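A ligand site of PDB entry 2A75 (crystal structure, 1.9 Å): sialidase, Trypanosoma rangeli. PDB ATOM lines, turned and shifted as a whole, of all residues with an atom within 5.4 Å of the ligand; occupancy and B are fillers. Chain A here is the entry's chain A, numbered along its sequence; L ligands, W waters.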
ATOM      1  N   ARG A  50      16.852  19.903  15.886  1.00  0.00           N
ATOM      2  CA  ARG A  50      17.857  19.838  14.817  1.00  0.00           C
ATOM      3  C   ARG A  50      19.078  19.033  15.242  1.00  0.00           C
ATOM      4  O   ARG A  50      19.151  18.558  16.367  1.00  0.00           O
ATOM      5  CB  ARG A  50      18.298  21.270  14.451  1.00  0.00           C
ATOM      6  CG  ARG A  50      17.281  22.165  13.704  1.00  0.00           C
ATOM      7  CD  ARG A  50      18.015  23.223  12.917  1.00  0.00           C
ATOM      8  NE  ARG A  50      18.869  22.524  11.952  1.00  0.00           N
ATOM      9  CZ  ARG A  50      19.934  23.055  11.352  1.00  0.00           C
ATOM     10  NH1 ARG A  50      20.652  22.306  10.501  1.00  0.00           N
ATOM     11  NH2 ARG A  50      20.263  24.312  11.589  1.00  0.00           N
ATOM     12  N   ILE A  51      20.030  18.888  14.329  1.00  0.00           N
ATOM     13  CA  ILE A  51      21.298  18.203  14.614  1.00  0.00           C
ATOM     14  C   ILE A  51      21.102  16.775  15.160  1.00  0.00           C
ATOM     15  O   ILE A  51      21.530  16.453  16.252  1.00  0.00           O
ATOM     16  CB  ILE A  51      22.114  19.009  15.632  1.00  0.00           C
ATOM     17  CG1 ILE A  51      21.799  20.512  15.476  1.00  0.00           C
ATOM     18  CG2 ILE A  51      23.621  18.718  15.470  1.00  0.00           C
ATOM     19  CD1 ILE A  51      22.044  21.081  14.018  1.00  0.00           C
ATOM     20  N   ASP A  66      19.413  18.707  19.119  1.00  0.00           N
ATOM     21  CA  ASP A  66      19.362  20.061  19.675  1.00  0.00           C
ATOM     22  C   ASP A  66      17.849  20.306  19.866  1.00  0.00           C
ATOM     23  O   ASP A  66      17.072  20.071  18.927  1.00  0.00           O
ATOM     24  CB  ASP A  66      19.737  21.121  18.649  1.00  0.00           C
ATOM     25  CG  ASP A  66      21.223  21.495  18.650  1.00  0.00           C
ATOM     26  OD1 ASP A  66      22.108  20.705  19.084  1.00  0.00           O
ATOM     27  OD2 ASP A  66      21.483  22.628  18.149  1.00  0.00           O
ATOM     28  N   ARG A  68      15.802  23.309  20.133  1.00  0.00           N
ATOM     29  CA  ARG A  68      15.890  24.763  20.026  1.00  0.00           C
ATOM     30  C   ARG A  68      14.475  25.221  20.384  1.00  0.00           C
ATOM     31  O   ARG A  68      13.578  25.283  19.563  1.00  0.00           O
ATOM     32  CB  ARG A  68      16.288  25.140  18.623  1.00  0.00           C
ATOM     33  CG  ARG A  68      17.542  24.371  18.170  1.00  0.00           C
ATOM     34  CD  ARG A  68      18.179  24.955  16.912  1.00  0.00           C
ATOM     35  NE  ARG A  68      19.530  24.400  16.732  1.00  0.00           N
ATOM     36  CZ  ARG A  68      20.403  24.781  15.811  1.00  0.00           C
ATOM     37  NH1 ARG A  68      20.096  25.732  14.945  1.00  0.00           N
ATOM     38  NH2 ARG A  68      21.646  24.210  15.771  1.00  0.00           N
ATOM     39  N   ASP A  74      20.603  29.435  15.111  1.00  0.00           N
ATOM     40  CA  ASP A  74      21.744  28.851  15.829  1.00  0.00           C
ATOM     41  C   ASP A  74      22.035  29.576  17.139  1.00  0.00           C
ATOM     42  O   ASP A  74      22.391  28.966  18.127  1.00  0.00           O
ATOM     43  CB  ASP A  74      23.024  28.912  14.979  1.00  0.00           C
ATOM     44  CG  ASP A  74      22.908  28.116  13.707  1.00  0.00           C
ATOM     45  OD1 ASP A  74      23.779  28.318  12.823  1.00  0.00           O
ATOM     46  OD2 ASP A  74      21.966  27.298  13.570  1.00  0.00           O
ATOM     47  N   MET A 110      25.121  22.950  22.114  1.00  0.00           N
ATOM     48  CA  MET A 110      24.709  22.520  20.801  1.00  0.00           C
ATOM     49  C   MET A 110      25.695  21.654  20.008  1.00  0.00           C
ATOM     50  O   MET A 110      26.849  21.478  20.403  1.00  0.00           O
ATOM     51  CB  MET A 110      24.375  23.784  20.001  1.00  0.00           C
ATOM     52  CG  MET A 110      25.616  24.649  19.600  1.00  0.00           C
ATOM     53  SD  MET A 110      25.161  26.366  19.117  1.00  0.00           S
ATOM     54  CE  MET A 110      24.196  26.038  17.516  1.00  0.00           C
ATOM     55  N   ASP A 111      25.184  21.111  18.899  1.00  0.00           N
ATOM     56  CA  ASP A 111      25.961  20.303  17.950  1.00  0.00           C
ATOM     57  C   ASP A 111      26.634  19.076  18.543  1.00  0.00           C
ATOM     58  O   ASP A 111      27.852  18.892  18.426  1.00  0.00           O
ATOM     59  CB  ASP A 111      27.029  21.157  17.276  1.00  0.00           C
ATOM     60  CG  ASP A 111      26.447  22.173  16.283  1.00  0.00           C
ATOM     61  OD1 ASP A 111      25.193  22.230  16.113  1.00  0.00           O
ATOM     62  OD2 ASP A 111      27.251  22.909  15.681  1.00  0.00           O
ATOM     63  N   PHE A 128      27.644  27.906  24.789  1.00  0.00           N
ATOM     64  CA  PHE A 128      27.784  29.365  24.669  1.00  0.00           C
ATOM     65  C   PHE A 128      26.834  30.048  25.658  1.00  0.00           C
ATOM     66  O   PHE A 128      25.750  29.515  25.969  1.00  0.00           O
ATOM     67  CB  PHE A 128      27.456  29.806  23.230  1.00  0.00           C
ATOM     68  CG  PHE A 128      28.323  29.153  22.186  1.00  0.00           C
ATOM     69  CD1 PHE A 128      28.026  27.872  21.718  1.00  0.00           C
ATOM     70  CD2 PHE A 128      29.467  29.788  21.740  1.00  0.00           C
ATOM     71  CE1 PHE A 128      28.895  27.219  20.808  1.00  0.00           C
ATOM     72  CE2 PHE A 128      30.341  29.141  20.837  1.00  0.00           C
ATOM     73  CZ  PHE A 128      30.041  27.854  20.376  1.00  0.00           C
ATOM     74  N   SER A 134      27.795  34.067  14.928  1.00  0.00           N
ATOM     75  CA  SER A 134      28.355  32.733  14.709  1.00  0.00           C
ATOM     76  C   SER A 134      29.698  32.483  15.411  1.00  0.00           C
ATOM     77  O   SER A 134      30.574  33.364  15.433  1.00  0.00           O
ATOM     78  CB  SER A 134      28.500  32.523  13.186  1.00  0.00           C
ATOM     79  OG  SER A 134      28.274  31.149  12.838  1.00  0.00           O
ATOM     80  N   TRP A 135      29.868  31.259  15.916  1.00  0.00           N
ATOM     81  CA  TRP A 135      31.091  30.906  16.659  1.00  0.00           C
ATOM     82  C   TRP A 135      32.384  31.238  15.942  1.00  0.00           C
ATOM     83  O   TRP A 135      33.302  31.747  16.567  1.00  0.00           O
ATOM     84  CB  TRP A 135      31.071  29.401  17.051  1.00  0.00           C
ATOM     85  CG  TRP A 135      31.285  28.441  15.922  1.00  0.00           C
ATOM     86  CD1 TRP A 135      30.442  28.167  14.869  1.00  0.00           C
ATOM     87  CD2 TRP A 135      32.427  27.576  15.773  1.00  0.00           C
ATOM     88  NE1 TRP A 135      31.000  27.171  14.080  1.00  0.00           N
ATOM     89  CE2 TRP A 135      32.208  26.794  14.612  1.00  0.00           C
ATOM     90  CE3 TRP A 135      33.598  27.391  16.515  1.00  0.00           C
ATOM     91  CZ2 TRP A 135      33.138  25.831  14.173  1.00  0.00           C
ATOM     92  CZ3 TRP A 135      34.529  26.428  16.090  1.00  0.00           C
ATOM     93  CH2 TRP A 135      34.280  25.657  14.911  1.00  0.00           C
ATOM     94  N   THR A 136      32.458  31.018  14.633  1.00  0.00           N
ATOM     95  CA  THR A 136      33.704  31.333  13.936  1.00  0.00           C
ATOM     96  C   THR A 136      34.001  32.843  13.898  1.00  0.00           C
ATOM     97  O   THR A 136      35.157  33.248  13.736  1.00  0.00           O
ATOM     98  CB  THR A 136      33.715  30.830  12.450  1.00  0.00           C
ATOM     99  OG1 THR A 136      32.680  31.494  11.706  1.00  0.00           O
ATOM    100  CG2 THR A 136      33.485  29.325  12.388  1.00  0.00           C
ATOM    101  N   ILE A 191      34.811  22.695  18.321  1.00  0.00           N
ATOM    102  CA  ILE A 191      33.600  21.944  18.582  1.00  0.00           C
ATOM    103  C   ILE A 191      33.796  20.548  17.926  1.00  0.00           C
ATOM    104  O   ILE A 191      34.698  20.357  17.090  1.00  0.00           O
ATOM    105  CB  ILE A 191      32.408  22.684  17.934  1.00  0.00           C
ATOM    106  CG1 ILE A 191      32.208  24.035  18.633  1.00  0.00           C
ATOM    107  CG2 ILE A 191      31.154  21.893  18.065  1.00  0.00           C
ATOM    108  CD1 ILE A 191      31.308  25.037  17.781  1.00  0.00           C
ATOM    109  N   GLN A 210      36.367  20.454  14.746  1.00  0.00           N
ATOM    110  CA  GLN A 210      36.490  21.609  13.854  1.00  0.00           C
ATOM    111  C   GLN A 210      37.017  22.752  14.760  1.00  0.00           C
ATOM    112  O   GLN A 210      36.488  23.027  15.841  1.00  0.00           O
ATOM    113  CB  GLN A 210      35.125  21.988  13.239  1.00  0.00           C
ATOM    114  CG  GLN A 210      33.927  21.661  14.110  1.00  0.00           C
ATOM    115  CD  GLN A 210      32.585  21.958  13.443  1.00  0.00           C
ATOM    116  OE1 GLN A 210      31.521  21.560  13.972  1.00  0.00           O
ATOM    117  NE2 GLN A 210      32.613  22.628  12.286  1.00  0.00           N
ATOM    118  N   SER A 244      35.076  21.824   7.676  1.00  0.00           N
ATOM    119  CA  SER A 244      34.346  21.865   8.929  1.00  0.00           C
ATOM    120  C   SER A 244      33.564  20.568   9.139  1.00  0.00           C
ATOM    121  O   SER A 244      33.679  19.628   8.340  1.00  0.00           O
ATOM    122  CB  SER A 244      33.387  23.069   8.964  1.00  0.00           C
ATOM    123  OG  SER A 244      32.503  23.036   7.851  1.00  0.00           O
ATOM    124  N   GLU A 245      32.760  20.516  10.208  1.00  0.00           N
ATOM    125  CA  GLU A 245      31.944  19.353  10.585  1.00  0.00           C
ATOM    126  C   GLU A 245      32.503  18.029  10.052  1.00  0.00           C
ATOM    127  O   GLU A 245      31.902  17.360   9.181  1.00  0.00           O
ATOM    128  CB  GLU A 245      30.473  19.559  10.138  1.00  0.00           C
ATOM    129  CG  GLU A 245      29.824  20.746  10.873  1.00  0.00           C
ATOM    130  CD  GLU A 245      28.375  20.988  10.517  1.00  0.00           C
ATOM    131  OE1 GLU A 245      27.957  20.663   9.375  1.00  0.00           O
ATOM    132  OE2 GLU A 245      27.653  21.541  11.390  1.00  0.00           O
ATOM    133  N   ARG A 260      32.980  18.658   5.795  1.00  0.00           N
ATOM    134  CA  ARG A 260      32.043  19.558   5.182  1.00  0.00           C
ATOM    135  C   ARG A 260      32.941  20.657   4.619  1.00  0.00           C
ATOM    136  O   ARG A 260      33.952  21.038   5.240  1.00  0.00           O
ATOM    137  CB  ARG A 260      31.080  20.148   6.216  1.00  0.00           C
ATOM    138  CG  ARG A 260      30.211  21.285   5.680  1.00  0.00           C
ATOM    139  CD  ARG A 260      29.263  21.870   6.769  1.00  0.00           C
ATOM    140  NE  ARG A 260      28.648  23.120   6.340  1.00  0.00           N
ATOM    141  CZ  ARG A 260      27.593  23.680   6.936  1.00  0.00           C
ATOM    142  NH1 ARG A 260      27.038  23.072   7.973  1.00  0.00           N
ATOM    143  NH2 ARG A 260      27.103  24.860   6.522  1.00  0.00           N
ATOM    144  N   ASP A 262      32.066  24.288   2.872  1.00  0.00           N
ATOM    145  CA  ASP A 262      31.154  25.257   2.256  1.00  0.00           C
ATOM    146  C   ASP A 262      31.780  25.846   0.970  1.00  0.00           C
ATOM    147  O   ASP A 262      32.956  26.206   0.955  1.00  0.00           O
ATOM    148  CB  ASP A 262      30.876  26.390   3.235  1.00  0.00           C
ATOM    149  CG  ASP A 262      30.113  25.911   4.465  1.00  0.00           C
ATOM    150  OD1 ASP A 262      30.435  26.381   5.580  1.00  0.00           O
ATOM    151  OD2 ASP A 262      29.192  25.075   4.297  1.00  0.00           O
ATOM    152  N   GLN A 298      26.473  26.599   0.254  1.00  0.00           N
ATOM    153  CA  GLN A 298      26.673  26.274   1.671  1.00  0.00           C
ATOM    154  C   GLN A 298      26.611  24.733   1.683  1.00  0.00           C
ATOM    155  O   GLN A 298      25.723  24.149   1.041  1.00  0.00           O
ATOM    156  CB  GLN A 298      25.467  26.865   2.396  1.00  0.00           C
ATOM    157  CG  GLN A 298      25.415  26.936   3.881  1.00  0.00           C
ATOM    158  CD  GLN A 298      24.134  27.705   4.309  1.00  0.00           C
ATOM    159  OE1 GLN A 298      23.768  27.713   5.486  1.00  0.00           O
ATOM    160  NE2 GLN A 298      23.484  28.370   3.338  1.00  0.00           N
ATOM    161  N   ASP A 299      27.538  24.082   2.374  1.00  0.00           N
ATOM    162  CA  ASP A 299      27.513  22.621   2.411  1.00  0.00           C
ATOM    163  C   ASP A 299      26.655  22.218   3.629  1.00  0.00           C
ATOM    164  O   ASP A 299      26.041  23.087   4.297  1.00  0.00           O
ATOM    165  CB  ASP A 299      28.948  22.073   2.513  1.00  0.00           C
ATOM    166  CG  ASP A 299      29.054  20.552   2.216  1.00  0.00           C
ATOM    167  OD1 ASP A 299      28.057  19.855   1.907  1.00  0.00           O
ATOM    168  OD2 ASP A 299      30.191  20.052   2.329  1.00  0.00           O
ATOM    169  N   ARG A 329      18.616  22.167   1.334  1.00  0.00           N
ATOM    170  CA  ARG A 329      19.035  20.772   1.485  1.00  0.00           C
ATOM    171  C   ARG A 329      17.962  19.712   1.186  1.00  0.00           C
ATOM    172  O   ARG A 329      17.754  18.782   1.958  1.00  0.00           O
ATOM    173  CB  ARG A 329      19.539  20.596   2.897  1.00  0.00           C
ATOM    174  CG  ARG A 329      20.836  21.377   3.123  1.00  0.00           C
ATOM    175  CD  ARG A 329      21.002  21.757   4.555  1.00  0.00           C
ATOM    176  NE  ARG A 329      22.247  22.492   4.724  1.00  0.00           N
ATOM    177  CZ  ARG A 329      22.578  23.147   5.838  1.00  0.00           C
ATOM    178  NH1 ARG A 329      21.759  23.129   6.886  1.00  0.00           N
ATOM    179  NH2 ARG A 329      23.698  23.847   5.884  1.00  0.00           N
ATOM    180  N   TYR A 357      20.560  18.030   8.215  1.00  0.00           N
ATOM    181  CA  TYR A 357      21.573  17.205   8.919  1.00  0.00           C
ATOM    182  C   TYR A 357      20.948  15.802   9.106  1.00  0.00           C
ATOM    183  O   TYR A 357      19.731  15.668   9.181  1.00  0.00           O
ATOM    184  CB  TYR A 357      21.935  17.849  10.279  1.00  0.00           C
ATOM    185  CG  TYR A 357      22.885  19.064  10.229  1.00  0.00           C
ATOM    186  CD1 TYR A 357      22.826  20.007   9.186  1.00  0.00           C
ATOM    187  CD2 TYR A 357      23.788  19.304  11.268  1.00  0.00           C
ATOM    188  CE1 TYR A 357      23.648  21.172   9.214  1.00  0.00           C
ATOM    189  CE2 TYR A 357      24.599  20.469  11.304  1.00  0.00           C
ATOM    190  CZ  TYR A 357      24.530  21.412  10.284  1.00  0.00           C
ATOM    191  OH  TYR A 357      25.235  22.619  10.438  1.00  0.00           O
HETATM  192  C1  LIG L   1      23.805  24.278   9.449  1.00  0.00           C
HETATM  193  F1  LIG L   1      23.138  25.023  12.107  1.00  0.00           F
HETATM  194  C2  LIG L   1      24.683  23.912  10.657  1.00  0.00           C
HETATM  195  C3  LIG L   1      23.905  23.943  12.000  1.00  0.00           C
HETATM  196  C4  LIG L   1      24.862  23.940  13.212  1.00  0.00           C
HETATM  197  O1  LIG L   1      24.161  23.940  14.447  1.00  0.00           O
HETATM  198  C5  LIG L   1      25.831  25.132  13.153  1.00  0.00           C
HETATM  199  N1  LIG L   1      26.666  25.084  14.236  1.00  0.00           N
HETATM  200  C6  LIG L   1      26.611  24.969  11.803  1.00  0.00           C
HETATM  201  O2  LIG L   1      25.675  24.932  10.702  1.00  0.00           O
HETATM  202  C7  LIG L   1      27.593  26.115  11.593  1.00  0.00           C
HETATM  203  O3  LIG L   1      26.812  27.289  11.751  1.00  0.00           O
HETATM  204  C8  LIG L   1      28.242  26.138  10.193  1.00  0.00           C
HETATM  205  O4  LIG L   1      29.098  25.010  10.076  1.00  0.00           O
HETATM  206  C9  LIG L   1      29.077  27.406   9.984  1.00  0.00           C
HETATM  207  O5  LIG L   1      30.088  27.528  10.969  1.00  0.00           O
HETATM  208  C10 LIG L   1      27.057  26.175  14.908  1.00  0.00           C
HETATM  209  O6  LIG L   1      26.825  27.318  14.488  1.00  0.00           O
HETATM  210  C11 LIG L   1      27.815  25.989  16.200  1.00  0.00           C
HETATM  211  O7  LIG L   1      24.384  24.731   8.425  1.00  0.00           O
HETATM  212  O8  LIG L   1      22.575  24.116   9.483  1.00  0.00           O
HETATM  213  O   HOH W   1      23.941  27.711  10.311  1.00  0.00           O
HETATM  214  O   HOH W   2      27.366  29.647  15.958  1.00  0.00           O
HETATM  215  O   HOH W   3      30.518  24.494  12.385  1.00  0.00           O
HETATM  216  O   HOH W   4      32.260  26.627   9.785  1.00  0.00           O
HETATM  217  O   HOH W   5      30.583  25.109   7.959  1.00  0.00           O
HETATM  218  O   HOH W   6      30.230  30.105  11.649  1.00  0.00           O
HETATM  219  O   HOH W   7      21.191  27.443  10.986  1.00  0.00           O
HETATM  220  O   HOH W   8      21.541  26.280   8.549  1.00  0.00           O
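Ile 51 touches the ligand (CD1 to O1, 3.6 Å).
Met 110 touches the ligand.
Ile 191 touches the ligand (CD1 to C11, 3.95 Å).
Glu 245 touches the ligand (OE2 to C6, 3.6 Å).
12 residues have an atom within 4 Å of the ligand: Arg 50, Ile 51, Arg 68, Asp 74, Met 110, Asp 111, Trp 135, Ile 191, Glu 245, Arg 260, Arg 329 and Tyr 357.
The nearest printed residue that does not touch the ligand is Thr 136 (4.1 Å).
Water W5 lies within hydrogen-bond range of O4 of the ligand, OD1 of Asp 262, OG of Ser 244 and NE of Arg 260.
Water W6 lies within hydrogen-bond range of OG of Ser 134 (2.5 Å), O5 of the ligand (2.7 Å) and OG1 of Thr 136 (2.8 Å).
Water W3 lies within hydrogen-bond range of O4 of the ligand (2.8 Å), NE2 of Gln 210 (2.8 Å) and NE1 of Trp 135 (3.2 Å).
Water W2 bridges an oxygen (O6) of the ligand (2.8 Å) and the backbone NH (N) of Trp 135 (3.0 Å).
Water W1 lies within hydrogen-bond range of the side-chain carboxylate of Asp 74 and an oxygen (O3) of the ligand.
Water W7 lies within hydrogen-bond range of OD2 of Asp 74 (2.7 Å) and NH2 of Arg 50 (3.3 Å).
The side-chain hydroxyl of Tyr 357 is bonded to a carbon (C2) of the ligand (1.4 Å).
O1 of the ligand sits at hydrogen-bond distance from OD1 of Asp 111 (2.6 Å).
The guanidinium group (NH2) of Arg 329 lies within salt-bridge range of an oxygen (O7) of the ligand (2.8 Å).
The guanidinium group (NH1) of Arg 50 lies within salt-bridge range of an oxygen (O8) of the ligand.
The guanidinium group (NH2) of Arg 68 is in hydrogen-bond range of an oxygen (O1) of the ligand (2.9 Å).
An oxygen (O3) of the ligand is in hydrogen-bond range of the side-chain carboxylate (OD1) of Asp 74, at 3.4 Å.
NH1 of Arg 260 lies within salt-bridge range of O7 of the ligand, at 3.2 Å.
NE1 of Trp 135 sits at hydrogen-bond distance from O5 of the ligand (3.3 Å).
The side-chain carboxylate (OD1) of Asp 66 is in hydrogen-bond range of the backbone NH (N) of Asp 111.
O of Asp 299 lies within hydrogen-bond range of NH2 of Arg 329 (2.9 Å).
OE1 of Glu 245 lies within salt-bridge range of NH1 of Arg 260, 2.9 Å away.
O of Arg 260 sits at hydrogen-bond distance from N of Ser 244 (2.8 Å).
The side-chain carboxylate of Asp 262 lies within salt-bridge range of the guanidinium group of Arg 260, 2.9 Å away.
NH2 of Arg 260 lies within hydrogen-bond range of O of Asp 299 (3.0 Å).
The side-chain amide nitrogen (NE2) of Gln 210 lies close to the backbone NH (N) of Glu 245.
O of Ile 191 lies within hydrogen-bond range of N of Gln 210, 2.9 Å away.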
